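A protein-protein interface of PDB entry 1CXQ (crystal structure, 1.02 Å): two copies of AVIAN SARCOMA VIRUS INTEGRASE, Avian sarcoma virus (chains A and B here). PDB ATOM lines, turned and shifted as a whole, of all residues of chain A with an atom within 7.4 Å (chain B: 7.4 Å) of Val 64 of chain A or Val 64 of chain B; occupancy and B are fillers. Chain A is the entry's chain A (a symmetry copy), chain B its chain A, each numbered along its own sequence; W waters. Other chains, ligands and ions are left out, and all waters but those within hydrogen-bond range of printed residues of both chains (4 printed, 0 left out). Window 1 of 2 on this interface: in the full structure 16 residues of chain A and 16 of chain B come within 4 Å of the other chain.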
ATOM      1  N   TRP A  14       8.529  27.214  -9.605  1.00  0.00           N
ATOM      2  CA  TRP A  14       8.235  26.950  -8.217  1.00  0.00           C
ATOM      3  C   TRP A  14       7.093  27.801  -7.728  1.00  0.00           C
ATOM      4  O   TRP A  14       6.816  28.874  -8.294  1.00  0.00           O
ATOM      5  CB  TRP A  14       9.452  27.309  -7.338  1.00  0.00           C
ATOM      6  CG  TRP A  14      10.684  26.531  -7.573  1.00  0.00           C
ATOM      7  CD1 TRP A  14      10.884  25.454  -8.377  1.00  0.00           C
ATOM      8  CD2 TRP A  14      11.941  26.820  -6.958  1.00  0.00           C
ATOM      9  NE1 TRP A  14      12.190  25.018  -8.279  1.00  0.00           N
ATOM     10  CE2 TRP A  14      12.864  25.867  -7.431  1.00  0.00           C
ATOM     11  CE3 TRP A  14      12.354  27.812  -6.064  1.00  0.00           C
ATOM     12  CZ2 TRP A  14      14.193  25.884  -7.016  1.00  0.00           C
ATOM     13  CZ3 TRP A  14      13.680  27.825  -5.668  1.00  0.00           C
ATOM     14  CH2 TRP A  14      14.592  26.852  -6.153  1.00  0.00           C
ATOM     15  N   ALA A  40       8.190  18.106  -5.511  1.00  0.00           N
ATOM     16  CA  ALA A  40       9.176  18.098  -4.409  1.00  0.00           C
ATOM     17  C   ALA A  40       8.991  19.376  -3.599  1.00  0.00           C
ATOM     18  O   ALA A  40       8.721  20.420  -4.161  1.00  0.00           O
ATOM     19  CB  ALA A  40      10.605  18.009  -4.912  1.00  0.00           C
ATOM     20  N   ILE A  41       9.228  19.261  -2.325  1.00  0.00           N
ATOM     21  CA  ILE A  41       9.161  20.387  -1.392  1.00  0.00           C
ATOM     22  C   ILE A  41      10.524  20.609  -0.754  1.00  0.00           C
ATOM     23  O   ILE A  41      11.256  19.690  -0.407  1.00  0.00           O
ATOM     24  CB  ILE A  41       8.068  20.032  -0.343  1.00  0.00           C
ATOM     25  CG1 ILE A  41       6.664  20.005  -0.971  1.00  0.00           C
ATOM     26  CG2 ILE A  41       8.045  20.895   0.905  1.00  0.00           C
ATOM     27  CD1 ILE A  41       5.667  19.249  -0.065  1.00  0.00           C
ATOM     28  N   VAL A  42      10.833  21.891  -0.543  1.00  0.00           N
ATOM     29  CA  VAL A  42      11.925  22.304   0.326  1.00  0.00           C
ATOM     30  C   VAL A  42      11.318  23.160   1.409  1.00  0.00           C
ATOM     31  O   VAL A  42      10.581  24.112   1.106  1.00  0.00           O
ATOM     32  CB  VAL A  42      13.010  23.074  -0.440  1.00  0.00           C
ATOM     33  CG1 VAL A  42      14.097  23.608   0.507  1.00  0.00           C
ATOM     34  CG2 VAL A  42      13.647  22.214  -1.516  1.00  0.00           C
ATOM     35  N   TRP A  58      15.399  30.491  -0.422  1.00  0.00           N
ATOM     36  CA  TRP A  58      15.601  30.160  -1.843  1.00  0.00           C
ATOM     37  C   TRP A  58      17.018  29.739  -2.107  1.00  0.00           C
ATOM     38  O   TRP A  58      17.240  28.888  -2.984  1.00  0.00           O
ATOM     39  CB  TRP A  58      15.194  31.346  -2.733  1.00  0.00           C
ATOM     40  CG  TRP A  58      13.730  31.512  -2.929  1.00  0.00           C
ATOM     41  CD1 TRP A  58      12.775  30.545  -3.065  1.00  0.00           C
ATOM     42  CD2 TRP A  58      13.041  32.766  -3.046  1.00  0.00           C
ATOM     43  NE1 TRP A  58      11.548  31.106  -3.266  1.00  0.00           N
ATOM     44  CE2 TRP A  58      11.679  32.473  -3.252  1.00  0.00           C
ATOM     45  CE3 TRP A  58      13.480  34.085  -3.001  1.00  0.00           C
ATOM     46  CZ2 TRP A  58      10.749  33.476  -3.402  1.00  0.00           C
ATOM     47  CZ3 TRP A  58      12.528  35.078  -3.160  1.00  0.00           C
ATOM     48  CH2 TRP A  58      11.188  34.772  -3.354  1.00  0.00           C
ATOM     49  N   ALA A  59      18.008  30.311  -1.421  1.00  0.00           N
ATOM     50  CA  ALA A  59      19.377  29.862  -1.631  1.00  0.00           C
ATOM     51  C   ALA A  59      19.464  28.355  -1.373  1.00  0.00           C
ATOM     52  O   ALA A  59      20.084  27.591  -2.124  1.00  0.00           O
ATOM     53  CB  ALA A  59      20.325  30.634  -0.741  1.00  0.00           C
ATOM     54  N   THR A  60      18.867  27.928  -0.265  1.00  0.00           N
ATOM     55  CA  THR A  60      18.843  26.499   0.060  1.00  0.00           C
ATOM     56  C   THR A  60      18.045  25.701  -0.956  1.00  0.00           C
ATOM     57  O   THR A  60      18.447  24.620  -1.388  1.00  0.00           O
ATOM     58  CB  THR A  60      18.267  26.313   1.487  1.00  0.00           C
ATOM     59  OG1 THR A  60      19.200  26.918   2.369  1.00  0.00           O
ATOM     60  CG2 THR A  60      18.054  24.877   1.821  1.00  0.00           C
ATOM     61  N   ALA A  61      16.881  26.229  -1.362  1.00  0.00           N
ATOM     62  CA  ALA A  61      16.070  25.514  -2.357  1.00  0.00           C
ATOM     63  C   ALA A  61      16.804  25.344  -3.664  1.00  0.00           C
ATOM     64  O   ALA A  61      16.687  24.286  -4.306  1.00  0.00           O
ATOM     65  CB  ALA A  61      14.735  26.208  -2.567  1.00  0.00           C
ATOM     66  N   ILE A  62      17.584  26.333  -4.096  1.00  0.00           N
ATOM     67  CA  ILE A  62      18.381  26.218  -5.327  1.00  0.00           C
ATOM     68  C   ILE A  62      19.434  25.124  -5.177  1.00  0.00           C
ATOM     69  O   ILE A  62      19.671  24.353  -6.110  1.00  0.00           O
ATOM     70  CB  ILE A  62      19.001  27.574  -5.689  1.00  0.00           C
ATOM     71  CG1 ILE A  62      17.929  28.592  -6.096  1.00  0.00           C
ATOM     72  CG2 ILE A  62      20.043  27.451  -6.756  1.00  0.00           C
ATOM     73  CD1 ILE A  62      18.446  30.019  -6.126  1.00  0.00           C
ATOM     74  N   ALA A  63      20.074  25.050  -4.013  1.00  0.00           N
ATOM     75  CA  ALA A  63      21.057  23.973  -3.757  1.00  0.00           C
ATOM     76  C   ALA A  63      20.419  22.620  -3.899  1.00  0.00           C
ATOM     77  O   ALA A  63      21.068  21.670  -4.394  1.00  0.00           O
ATOM     78  CB  ALA A  63      21.673  24.161  -2.408  1.00  0.00           C
ATOM     79  N   VAL A  64      19.175  22.461  -3.460  1.00  0.00           N
ATOM     80  CA  VAL A  64      18.488  21.188  -3.496  1.00  0.00           C
ATOM     81  C   VAL A  64      17.908  20.866  -4.866  1.00  0.00           C
ATOM     82  O   VAL A  64      18.081  19.764  -5.390  1.00  0.00           O
ATOM     83  CB  VAL A  64      17.389  21.157  -2.435  1.00  0.00           C
ATOM     84  CG1 VAL A  64      16.539  19.888  -2.554  1.00  0.00           C
ATOM     85  CG2 VAL A  64      17.990  21.290  -1.066  1.00  0.00           C
ATOM     86  N   LEU A  65      17.175  21.800  -5.452  1.00  0.00           N
ATOM     87  CA  LEU A  65      16.368  21.594  -6.635  1.00  0.00           C
ATOM     88  C   LEU A  65      16.976  22.078  -7.939  1.00  0.00           C
ATOM     89  O   LEU A  65      16.441  21.744  -9.021  1.00  0.00           O
ATOM     90  CB  LEU A  65      15.023  22.309  -6.444  1.00  0.00           C
ATOM     91  CG  LEU A  65      14.158  21.851  -5.280  1.00  0.00           C
ATOM     92  CD1 LEU A  65      12.972  22.793  -5.110  1.00  0.00           C
ATOM     93  CD2 LEU A  65      13.690  20.416  -5.481  1.00  0.00           C
ATOM     94  N   GLY A  66      17.994  22.904  -7.887  1.00  0.00           N
ATOM     95  CA  GLY A  66      18.514  23.572  -9.057  1.00  0.00           C
ATOM     96  C   GLY A  66      17.903  24.954  -9.189  1.00  0.00           C
ATOM     97  O   GLY A  66      17.030  25.371  -8.433  1.00  0.00           O
ATOM     98  N   ARG A  67      18.375  25.717 -10.160  1.00  0.00           N
ATOM     99  CA  ARG A  67      17.903  27.029 -10.374  1.00  0.00           C
ATOM    100  C   ARG A  67      16.640  27.001 -11.206  1.00  0.00           C
ATOM    101  O   ARG A  67      16.650  26.462 -12.329  1.00  0.00           O
ATOM    102  CB  ARG A  67      19.001  27.842 -11.072  1.00  0.00           C
ATOM    103  CG  ARG A  67      18.620  29.275 -11.171  1.00  0.00           C
ATOM    104  CD  ARG A  67      19.561  30.170 -11.895  1.00  0.00           C
ATOM    105  NE  ARG A  67      20.277  29.613 -12.946  1.00  0.00           N
ATOM    106  CZ  ARG A  67      21.359  30.337 -13.337  1.00  0.00           C
ATOM    107  NH1 ARG A  67      21.644  31.522 -12.755  1.00  0.00           N
ATOM    108  NH2 ARG A  67      22.087  29.855 -14.304  1.00  0.00           N
ATOM    109  N   ALA A 143      13.416  17.955   8.926  1.00  0.00           N
ATOM    110  CA  ALA A 143      14.011  17.193   7.837  1.00  0.00           C
ATOM    111  C   ALA A 143      13.276  15.885   7.607  1.00  0.00           C
ATOM    112  O   ALA A 143      13.126  15.446   6.451  1.00  0.00           O
ATOM    113  CB  ALA A 143      15.486  16.924   8.139  1.00  0.00           C
ATOM    114  N   MET A 146      10.138  16.650   5.627  1.00  0.00           N
ATOM    115  CA  MET A 146      10.477  16.900   4.257  1.00  0.00           C
ATOM    116  C   MET A 146      10.769  15.585   3.513  1.00  0.00           C
ATOM    117  O   MET A 146      10.300  15.351   2.403  1.00  0.00           O
ATOM    118  CB  MET A 146      11.669  17.839   4.177  1.00  0.00           C
ATOM    119  CG  MET A 146      12.118  18.222   2.776  1.00  0.00           C
ATOM    120  SD  MET A 146      13.355  19.507   2.843  1.00  0.00           S
ATOM    121  CE  MET A 146      14.208  19.220   1.289  1.00  0.00           C
ATOM    122  N   TYR A 147      11.586  14.717   4.144  1.00  0.00           N
ATOM    123  CA  TYR A 147      11.817  13.386   3.599  1.00  0.00           C
ATOM    124  C   TYR A 147      10.529  12.644   3.342  1.00  0.00           C
ATOM    125  O   TYR A 147      10.330  12.044   2.267  1.00  0.00           O
ATOM    126  CB  TYR A 147      12.698  12.592   4.590  1.00  0.00           C
ATOM    127  CG  TYR A 147      12.524  11.097   4.501  1.00  0.00           C
ATOM    128  CD1 TYR A 147      13.041  10.336   3.480  1.00  0.00           C
ATOM    129  CD2 TYR A 147      11.813  10.440   5.490  1.00  0.00           C
ATOM    130  CE1 TYR A 147      12.841   8.950   3.441  1.00  0.00           C
ATOM    131  CE2 TYR A 147      11.634   9.065   5.472  1.00  0.00           C
ATOM    132  CZ  TYR A 147      12.157   8.336   4.448  1.00  0.00           C
ATOM    133  OH  TYR A 147      12.009   6.961   4.384  1.00  0.00           O
ATOM    134  N   ASN A 150       8.701  13.917   0.294  1.00  0.00           N
ATOM    135  CA  ASN A 150       9.428  13.909  -0.982  1.00  0.00           C
ATOM    136  C   ASN A 150       9.817  12.556  -1.536  1.00  0.00           C
ATOM    137  O   ASN A 150       9.978  12.406  -2.740  1.00  0.00           O
ATOM    138  CB  ASN A 150      10.759  14.697  -0.994  1.00  0.00           C
ATOM    139  CG  ASN A 150      10.315  16.141  -0.848  1.00  0.00           C
ATOM    140  OD1 ASN A 150       9.236  16.651  -1.090  1.00  0.00           O
ATOM    141  ND2 ASN A 150      11.197  16.950  -0.410  1.00  0.00           N
ATOM    142  N   HIS A 151      10.129  11.609  -0.699  1.00  0.00           N
ATOM    143  CA  HIS A 151      10.778  10.340  -1.067  1.00  0.00           C
ATOM    144  C   HIS A 151       9.789   9.218  -0.810  1.00  0.00           C
ATOM    145  O   HIS A 151       9.394   8.982   0.340  1.00  0.00           O
ATOM    146  CB  HIS A 151      12.097  10.279  -0.265  1.00  0.00           C
ATOM    147  CG  HIS A 151      13.024  11.364  -0.692  1.00  0.00           C
ATOM    148  ND1 HIS A 151      13.594  11.425  -1.958  1.00  0.00           N
ATOM    149  CD2 HIS A 151      13.421  12.470   0.064  1.00  0.00           C
ATOM    150  CE1 HIS A 151      14.319  12.531  -1.994  1.00  0.00           C
ATOM    151  NE2 HIS A 151      14.205  13.132  -0.808  1.00  0.00           N
ATOM    152  N   TRP B  14      26.011   6.036  -0.067  1.00  0.00           N
ATOM    153  CA  TRP B  14      26.664   7.308   0.125  1.00  0.00           C
ATOM    154  C   TRP B  14      28.047   7.132   0.696  1.00  0.00           C
ATOM    155  O   TRP B  14      28.341   6.108   1.338  1.00  0.00           O
ATOM    156  CB  TRP B  14      25.878   8.160   1.145  1.00  0.00           C
ATOM    157  CG  TRP B  14      24.506   8.543   0.761  1.00  0.00           C
ATOM    158  CD1 TRP B  14      23.856   8.356  -0.417  1.00  0.00           C
ATOM    159  CD2 TRP B  14      23.588   9.203   1.634  1.00  0.00           C
ATOM    160  NE1 TRP B  14      22.586   8.894  -0.355  1.00  0.00           N
ATOM    161  CE2 TRP B  14      22.393   9.393   0.912  1.00  0.00           C
ATOM    162  CE3 TRP B  14      23.679   9.628   2.962  1.00  0.00           C
ATOM    163  CZ2 TRP B  14      21.290  10.013   1.495  1.00  0.00           C
ATOM    164  CZ3 TRP B  14      22.573  10.233   3.534  1.00  0.00           C
ATOM    165  CH2 TRP B  14      21.381  10.419   2.786  1.00  0.00           C
ATOM    166  N   ALA B  40      25.792  13.576  -6.619  1.00  0.00           N
ATOM    167  CA  ALA B  40      25.217  14.739  -5.910  1.00  0.00           C
ATOM    168  C   ALA B  40      25.896  14.846  -4.549  1.00  0.00           C
ATOM    169  O   ALA B  40      26.179  13.839  -3.929  1.00  0.00           O
ATOM    170  CB  ALA B  40      23.716  14.622  -5.730  1.00  0.00           C
ATOM    171  N   ILE B  41      26.050  16.058  -4.103  1.00  0.00           N
ATOM    172  CA  ILE B  41      26.626  16.363  -2.792  1.00  0.00           C
ATOM    173  C   ILE B  41      25.603  17.093  -1.937  1.00  0.00           C
ATOM    174  O   ILE B  41      24.847  17.949  -2.384  1.00  0.00           O
ATOM    175  CB  ILE B  41      27.898  17.221  -3.054  1.00  0.00           C
ATOM    176  CG1 ILE B  41      29.002  16.404  -3.748  1.00  0.00           C
ATOM    177  CG2 ILE B  41      28.479  17.926  -1.843  1.00  0.00           C
ATOM    178  CD1 ILE B  41      30.060  17.332  -4.384  1.00  0.00           C
ATOM    179  N   VAL B  42      25.635  16.773  -0.641  1.00  0.00           N
ATOM    180  CA  VAL B  42      24.973  17.567   0.383  1.00  0.00           C
ATOM    181  C   VAL B  42      26.045  18.015   1.345  1.00  0.00           C
ATOM    182  O   VAL B  42      26.825  17.183   1.835  1.00  0.00           O
ATOM    183  CB  VAL B  42      23.879  16.772   1.111  1.00  0.00           C
ATOM    184  CG1 VAL B  42      23.271  17.581   2.268  1.00  0.00           C
ATOM    185  CG2 VAL B  42      22.782  16.338   0.157  1.00  0.00           C
ATOM    186  N   TRP B  58      23.139  13.984   8.348  1.00  0.00           N
ATOM    187  CA  TRP B  58      22.443  12.928   7.595  1.00  0.00           C
ATOM    188  C   TRP B  58      20.960  13.164   7.569  1.00  0.00           C
ATOM    189  O   TRP B  58      20.311  12.817   6.569  1.00  0.00           O
ATOM    190  CB  TRP B  58      22.779  11.544   8.175  1.00  0.00           C
ATOM    191  CG  TRP B  58      24.112  11.008   7.791  1.00  0.00           C
ATOM    192  CD1 TRP B  58      24.765  11.127   6.597  1.00  0.00           C
ATOM    193  CD2 TRP B  58      24.965  10.214   8.630  1.00  0.00           C
ATOM    194  NE1 TRP B  58      25.954  10.460   6.631  1.00  0.00           N
ATOM    195  CE2 TRP B  58      26.108   9.893   7.873  1.00  0.00           C
ATOM    196  CE3 TRP B  58      24.833   9.758   9.937  1.00  0.00           C
ATOM    197  CZ2 TRP B  58      27.125   9.134   8.404  1.00  0.00           C
ATOM    198  CZ3 TRP B  58      25.865   8.991  10.450  1.00  0.00           C
ATOM    199  CH2 TRP B  58      26.989   8.690   9.693  1.00  0.00           C
ATOM    200  N   ALA B  59      20.368  13.708   8.633  1.00  0.00           N
ATOM    201  CA  ALA B  59      18.940  13.995   8.588  1.00  0.00           C
ATOM    202  C   ALA B  59      18.641  14.904   7.394  1.00  0.00           C
ATOM    203  O   ALA B  59      17.679  14.708   6.639  1.00  0.00           O
ATOM    204  CB  ALA B  59      18.490  14.621   9.890  1.00  0.00           C
ATOM    205  N   THR B  60      19.456  15.944   7.245  1.00  0.00           N
ATOM    206  CA  THR B  60      19.296  16.855   6.109  1.00  0.00           C
ATOM    207  C   THR B  60      19.562  16.160   4.785  1.00  0.00           C
ATOM    208  O   THR B  60      18.839  16.340   3.804  1.00  0.00           O
ATOM    209  CB  THR B  60      20.239  18.071   6.296  1.00  0.00           C
ATOM    210  OG1 THR B  60      19.766  18.760   7.444  1.00  0.00           O
ATOM    211  CG2 THR B  60      20.255  18.956   5.098  1.00  0.00           C
ATOM    212  N   ALA B  61      20.622  15.341   4.733  1.00  0.00           N
ATOM    213  CA  ALA B  61      20.924  14.625   3.486  1.00  0.00           C
ATOM    214  C   ALA B  61      19.801  13.702   3.081  1.00  0.00           C
ATOM    215  O   ALA B  61      19.500  13.586   1.880  1.00  0.00           O
ATOM    216  CB  ALA B  61      22.237  13.869   3.599  1.00  0.00           C
ATOM    217  N   ILE B  62      19.138  13.043   4.029  1.00  0.00           N
ATOM    218  CA  ILE B  62      17.991  12.175   3.719  1.00  0.00           C
ATOM    219  C   ILE B  62      16.842  12.999   3.145  1.00  0.00           C
ATOM    220  O   ILE B  62      16.178  12.571   2.198  1.00  0.00           O
ATOM    221  CB  ILE B  62      17.571  11.383   4.963  1.00  0.00           C
ATOM    222  CG1 ILE B  62      18.644  10.363   5.368  1.00  0.00           C
ATOM    223  CG2 ILE B  62      16.246  10.710   4.785  1.00  0.00           C
ATOM    224  CD1 ILE B  62      18.437   9.809   6.766  1.00  0.00           C
ATOM    225  N   ALA B  63      16.595  14.177   3.712  1.00  0.00           N
ATOM    226  CA  ALA B  63      15.547  15.072   3.171  1.00  0.00           C
ATOM    227  C   ALA B  63      15.827  15.420   1.737  1.00  0.00           C
ATOM    228  O   ALA B  63      14.882  15.535   0.924  1.00  0.00           O
ATOM    229  CB  ALA B  63      15.432  16.291   4.029  1.00  0.00           C
ATOM    230  N   VAL B  64      17.088  15.627   1.373  1.00  0.00           N
ATOM    231  CA  VAL B  64      17.462  16.022   0.032  1.00  0.00           C
ATOM    232  C   VAL B  64      17.511  14.851  -0.939  1.00  0.00           C
ATOM    233  O   VAL B  64      16.968  14.913  -2.044  1.00  0.00           O
ATOM    234  CB  VAL B  64      18.808  16.745   0.057  1.00  0.00           C
ATOM    235  CG1 VAL B  64      19.309  17.033  -1.362  1.00  0.00           C
ATOM    236  CG2 VAL B  64      18.703  18.003   0.869  1.00  0.00           C
ATOM    237  N   LEU B  65      18.195  13.780  -0.568  1.00  0.00           N
ATOM    238  CA  LEU B  65      18.535  12.676  -1.439  1.00  0.00           C
ATOM    239  C   LEU B  65      17.660  11.441  -1.310  1.00  0.00           C
ATOM    240  O   LEU B  65      17.755  10.536  -2.171  1.00  0.00           O
ATOM    241  CB  LEU B  65      19.988  12.259  -1.161  1.00  0.00           C
ATOM    242  CG  LEU B  65      21.062  13.308  -1.399  1.00  0.00           C
ATOM    243  CD1 LEU B  65      22.405  12.804  -0.881  1.00  0.00           C
ATOM    244  CD2 LEU B  65      21.150  13.673  -2.875  1.00  0.00           C
ATOM    245  N   GLY B  66      16.895  11.324  -0.251  1.00  0.00           N
ATOM    246  CA  GLY B  66      16.181  10.108   0.061  1.00  0.00           C
ATOM    247  C   GLY B  66      16.981   9.261   1.031  1.00  0.00           C
ATOM    248  O   GLY B  66      18.111   9.564   1.403  1.00  0.00           O
ATOM    249  N   ARG B  67      16.392   8.168   1.484  1.00  0.00           N
ATOM    250  CA  ARG B  67      17.025   7.307   2.405  1.00  0.00           C
ATOM    251  C   ARG B  67      17.933   6.341   1.678  1.00  0.00           C
ATOM    252  O   ARG B  67      17.467   5.599   0.793  1.00  0.00           O
ATOM    253  CB  ARG B  67      15.948   6.555   3.199  1.00  0.00           C
ATOM    254  CG  ARG B  67      16.556   5.760   4.297  1.00  0.00           C
ATOM    255  CD  ARG B  67      15.634   4.917   5.104  1.00  0.00           C
ATOM    256  NE  ARG B  67      14.531   4.386   4.450  1.00  0.00           N
ATOM    257  CZ  ARG B  67      13.548   3.939   5.274  1.00  0.00           C
ATOM    258  NH1 ARG B  67      13.699   3.982   6.616  1.00  0.00           N
ATOM    259  NH2 ARG B  67      12.474   3.451   4.720  1.00  0.00           N
ATOM    260  N   ALA B 143      25.403  27.308   0.237  1.00  0.00           N
ATOM    261  CA  ALA B 143      24.359  26.811  -0.648  1.00  0.00           C
ATOM    262  C   ALA B 143      24.711  27.042  -2.107  1.00  0.00           C
ATOM    263  O   ALA B 143      24.403  26.195  -2.966  1.00  0.00           O
ATOM    264  CB  ALA B 143      23.029  27.487  -0.312  1.00  0.00           C
ATOM    265  N   MET B 146      27.162  24.349  -3.151  1.00  0.00           N
ATOM    266  CA  MET B 146      26.470  23.107  -3.335  1.00  0.00           C
ATOM    267  C   MET B 146      25.706  23.095  -4.670  1.00  0.00           C
ATOM    268  O   MET B 146      25.749  22.135  -5.433  1.00  0.00           O
ATOM    269  CB  MET B 146      25.524  22.859  -2.172  1.00  0.00           C
ATOM    270  CG  MET B 146      24.747  21.553  -2.218  1.00  0.00           C
ATOM    271  SD  MET B 146      23.874  21.290  -0.683  1.00  0.00           S
ATOM    272  CE  MET B 146      22.540  20.227  -1.245  1.00  0.00           C
ATOM    273  N   TYR B 147      24.971  24.194  -4.941  1.00  0.00           N
ATOM    274  CA  TYR B 147      24.322  24.351  -6.235  1.00  0.00           C
ATOM    275  C   TYR B 147      25.291  24.199  -7.381  1.00  0.00           C
ATOM    276  O   TYR B 147      25.022  23.484  -8.367  1.00  0.00           O
ATOM    277  CB  TYR B 147      23.654  25.744  -6.287  1.00  0.00           C
ATOM    278  CG  TYR B 147      23.491  26.293  -7.682  1.00  0.00           C
ATOM    279  CD1 TYR B 147      22.541  25.839  -8.566  1.00  0.00           C
ATOM    280  CD2 TYR B 147      24.329  27.307  -8.111  1.00  0.00           C
ATOM    281  CE1 TYR B 147      22.440  26.378  -9.856  1.00  0.00           C
ATOM    282  CE2 TYR B 147      24.217  27.863  -9.376  1.00  0.00           C
ATOM    283  CZ  TYR B 147      23.267  27.394 -10.231  1.00  0.00           C
ATOM    284  OH  TYR B 147      23.112  27.916 -11.504  1.00  0.00           O
ATOM    285  N   ASN B 150      26.293  20.607  -7.969  1.00  0.00           N
ATOM    286  CA  ASN B 150      25.219  19.638  -8.223  1.00  0.00           C
ATOM    287  C   ASN B 150      24.416  19.830  -9.491  1.00  0.00           C
ATOM    288  O   ASN B 150      23.862  18.874 -10.019  1.00  0.00           O
ATOM    289  CB  ASN B 150      24.135  19.544  -7.123  1.00  0.00           C
ATOM    290  CG  ASN B 150      24.879  18.945  -5.945  1.00  0.00           C
ATOM    291  OD1 ASN B 150      25.908  18.294  -5.925  1.00  0.00           O
ATOM    292  ND2 ASN B 150      24.357  19.145  -4.800  1.00  0.00           N
ATOM    293  N   HIS B 151      24.199  21.042  -9.912  1.00  0.00           N
ATOM    294  CA  HIS B 151      23.228  21.410 -10.956  1.00  0.00           C
ATOM    295  C   HIS B 151      24.004  21.934 -12.150  1.00  0.00           C
ATOM    296  O   HIS B 151      24.683  22.966 -12.053  1.00  0.00           O
ATOM    297  CB  HIS B 151      22.241  22.401 -10.301  1.00  0.00           C
ATOM    298  CG  HIS B 151      21.462  21.732  -9.221  1.00  0.00           C
ATOM    299  ND1 HIS B 151      20.550  20.710  -9.461  1.00  0.00           N
ATOM    300  CD2 HIS B 151      21.548  21.983  -7.849  1.00  0.00           C
ATOM    301  CE1 HIS B 151      20.085  20.334  -8.281  1.00  0.00           C
ATOM    302  NE2 HIS B 151      20.680  21.084  -7.350  1.00  0.00           N
HETATM  303  O   HOH W   1      11.008   5.956   6.650  1.00  0.00           O
HETATM  304  O   HOH W   2      24.548  30.144 -11.854  1.00  0.00           O
HETATM  305  O   HOH W   3      22.135  28.540  -3.792  1.00  0.00           O
HETATM  306  O   HOH W   4      15.442  13.237   7.489  1.00  0.00           O
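O of Ala 63 of chain B sits at hydrogen-bond distance from NE2 of His 151 of chain A (3.0 Å).
The backbone NH (N) of Gly 66 of chain B lies within hydrogen-bond range of a ring nitrogen (NE2) of His 151 of chain A (3.3 Å).
NE2 of His 151 of chain B is in hydrogen-bond range of O of Ala 63 of chain A, 3.0 Å away.
The backbone NH of Gly 66 of chain A lies within hydrogen-bond range of a ring nitrogen (NE2) of His 151 of chain B (3.3 Å).
The backbone carbonyl oxygen (O) of Met 146 of chain B sits close to the side-chain amide nitrogen (ND2) of Asn 150 of chain B (3.4 Å).
O of Met 146 of chain A lies close to ND2 of Asn 150 of chain A (3.4 Å).
O of Ala 59 of chain A touches CB of Ala 143 of chain B, at 3.5 Å.
Ile 62 of chain A touches Tyr 147 of chain B.
His 151 of chain B touches Ile 62 of chain A.
Val 64 of chain A touches Val 64 of chain B.
Val 64 of chain A touches His 151 of chain B (O to NE2, 3.5 Å).
His 151 of chain B touches Leu 65 of chain A.
Ala 59 of chain B touches Ala 143 of chain A.
O of Ala 63 of chain B touches CE of Met 146 of chain A (3.8 Å).
CD1 of Tyr 147 of chain A touches CG2 of Ile 62 of chain B, at 3.5 Å.
Val 64 of chain A touches two residues of chain B.
Val 64 of chain B touches two residues of chain A.
Printed residues of chain A within 4 Å of Leu 65 of chain B: His 151 (3.6 Å).
Of the printed residues of chain A, Ala 59 of chain B touches Ala 143.
Printed residues of chain B within 4 Å of Met 146 of chain A: Ala 63 (3.8 Å).
Printed residues of chain B within 4 Å of Ala 63 of chain A: Ala 143, Met 146 and His 151.
Of the printed residues of chain A, Tyr 147 of chain B touches Ile 62 and Arg 67.
Trp 58 of chain B touches none of the printed residues of chain A.
Trp 14 of chain A touches none of the printed residues of chain B.
The nearest residue of chain B that does not touch Val 64 of chain A is Met 146 of chain B (4.6 Å).
Of the 19 printed residues of chain B, 11 touch a printed residue of chain A.
Hydrophobic or aromatic side chains of chain B within 4 Å of the printed part of chain A: Ile 62, Ala 63, Val 64, Ala 143, Met 146, Tyr 147 and His 151.
Along chain B the printed residues that touch a printed residue of chain A span positions 59 to 151.
Among the printed residues, no Asp or Glu carboxylate lies within 4 Å of a Lys or Arg side-chain nitrogen of the other chain.
Ala 59 of chain A touches Ala 143 of chain B, and with the chains exchanged Ala 143 of chain A touches Ala 59 of chain B.
Ala 63 of chain A touches His 151 of chain B, and with the chains exchanged His 151 of chain A touches Ala 63 of chain B.
Gly 66 of chain A touches His 151 of chain B, and with the chains exchanged His 151 of chain A touches Gly 66 of chain B.
Of the 21 pairs that touch across the chains among the printed residues, 21 have their exchanged pair printed and touching as well.
Water W2 bridges OH of Tyr 147 of chain B (2.7 Å) and NH1 of Arg 67 of chain A (3.3 Å).
Water W1 bridges OH of Tyr 147 of chain A (2.7 Å) and NH1 of Arg 67 of chain B (3.3 Å).
Water W4 lies within hydrogen-bond range of O of Ala 59 of chain B (2.8 Å) and O of Ala 143 of chain A (3.4 Å).
Water W3 lies within hydrogen-bond range of O of Ala 59 of chain A and O of Ala 143 of chain B.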
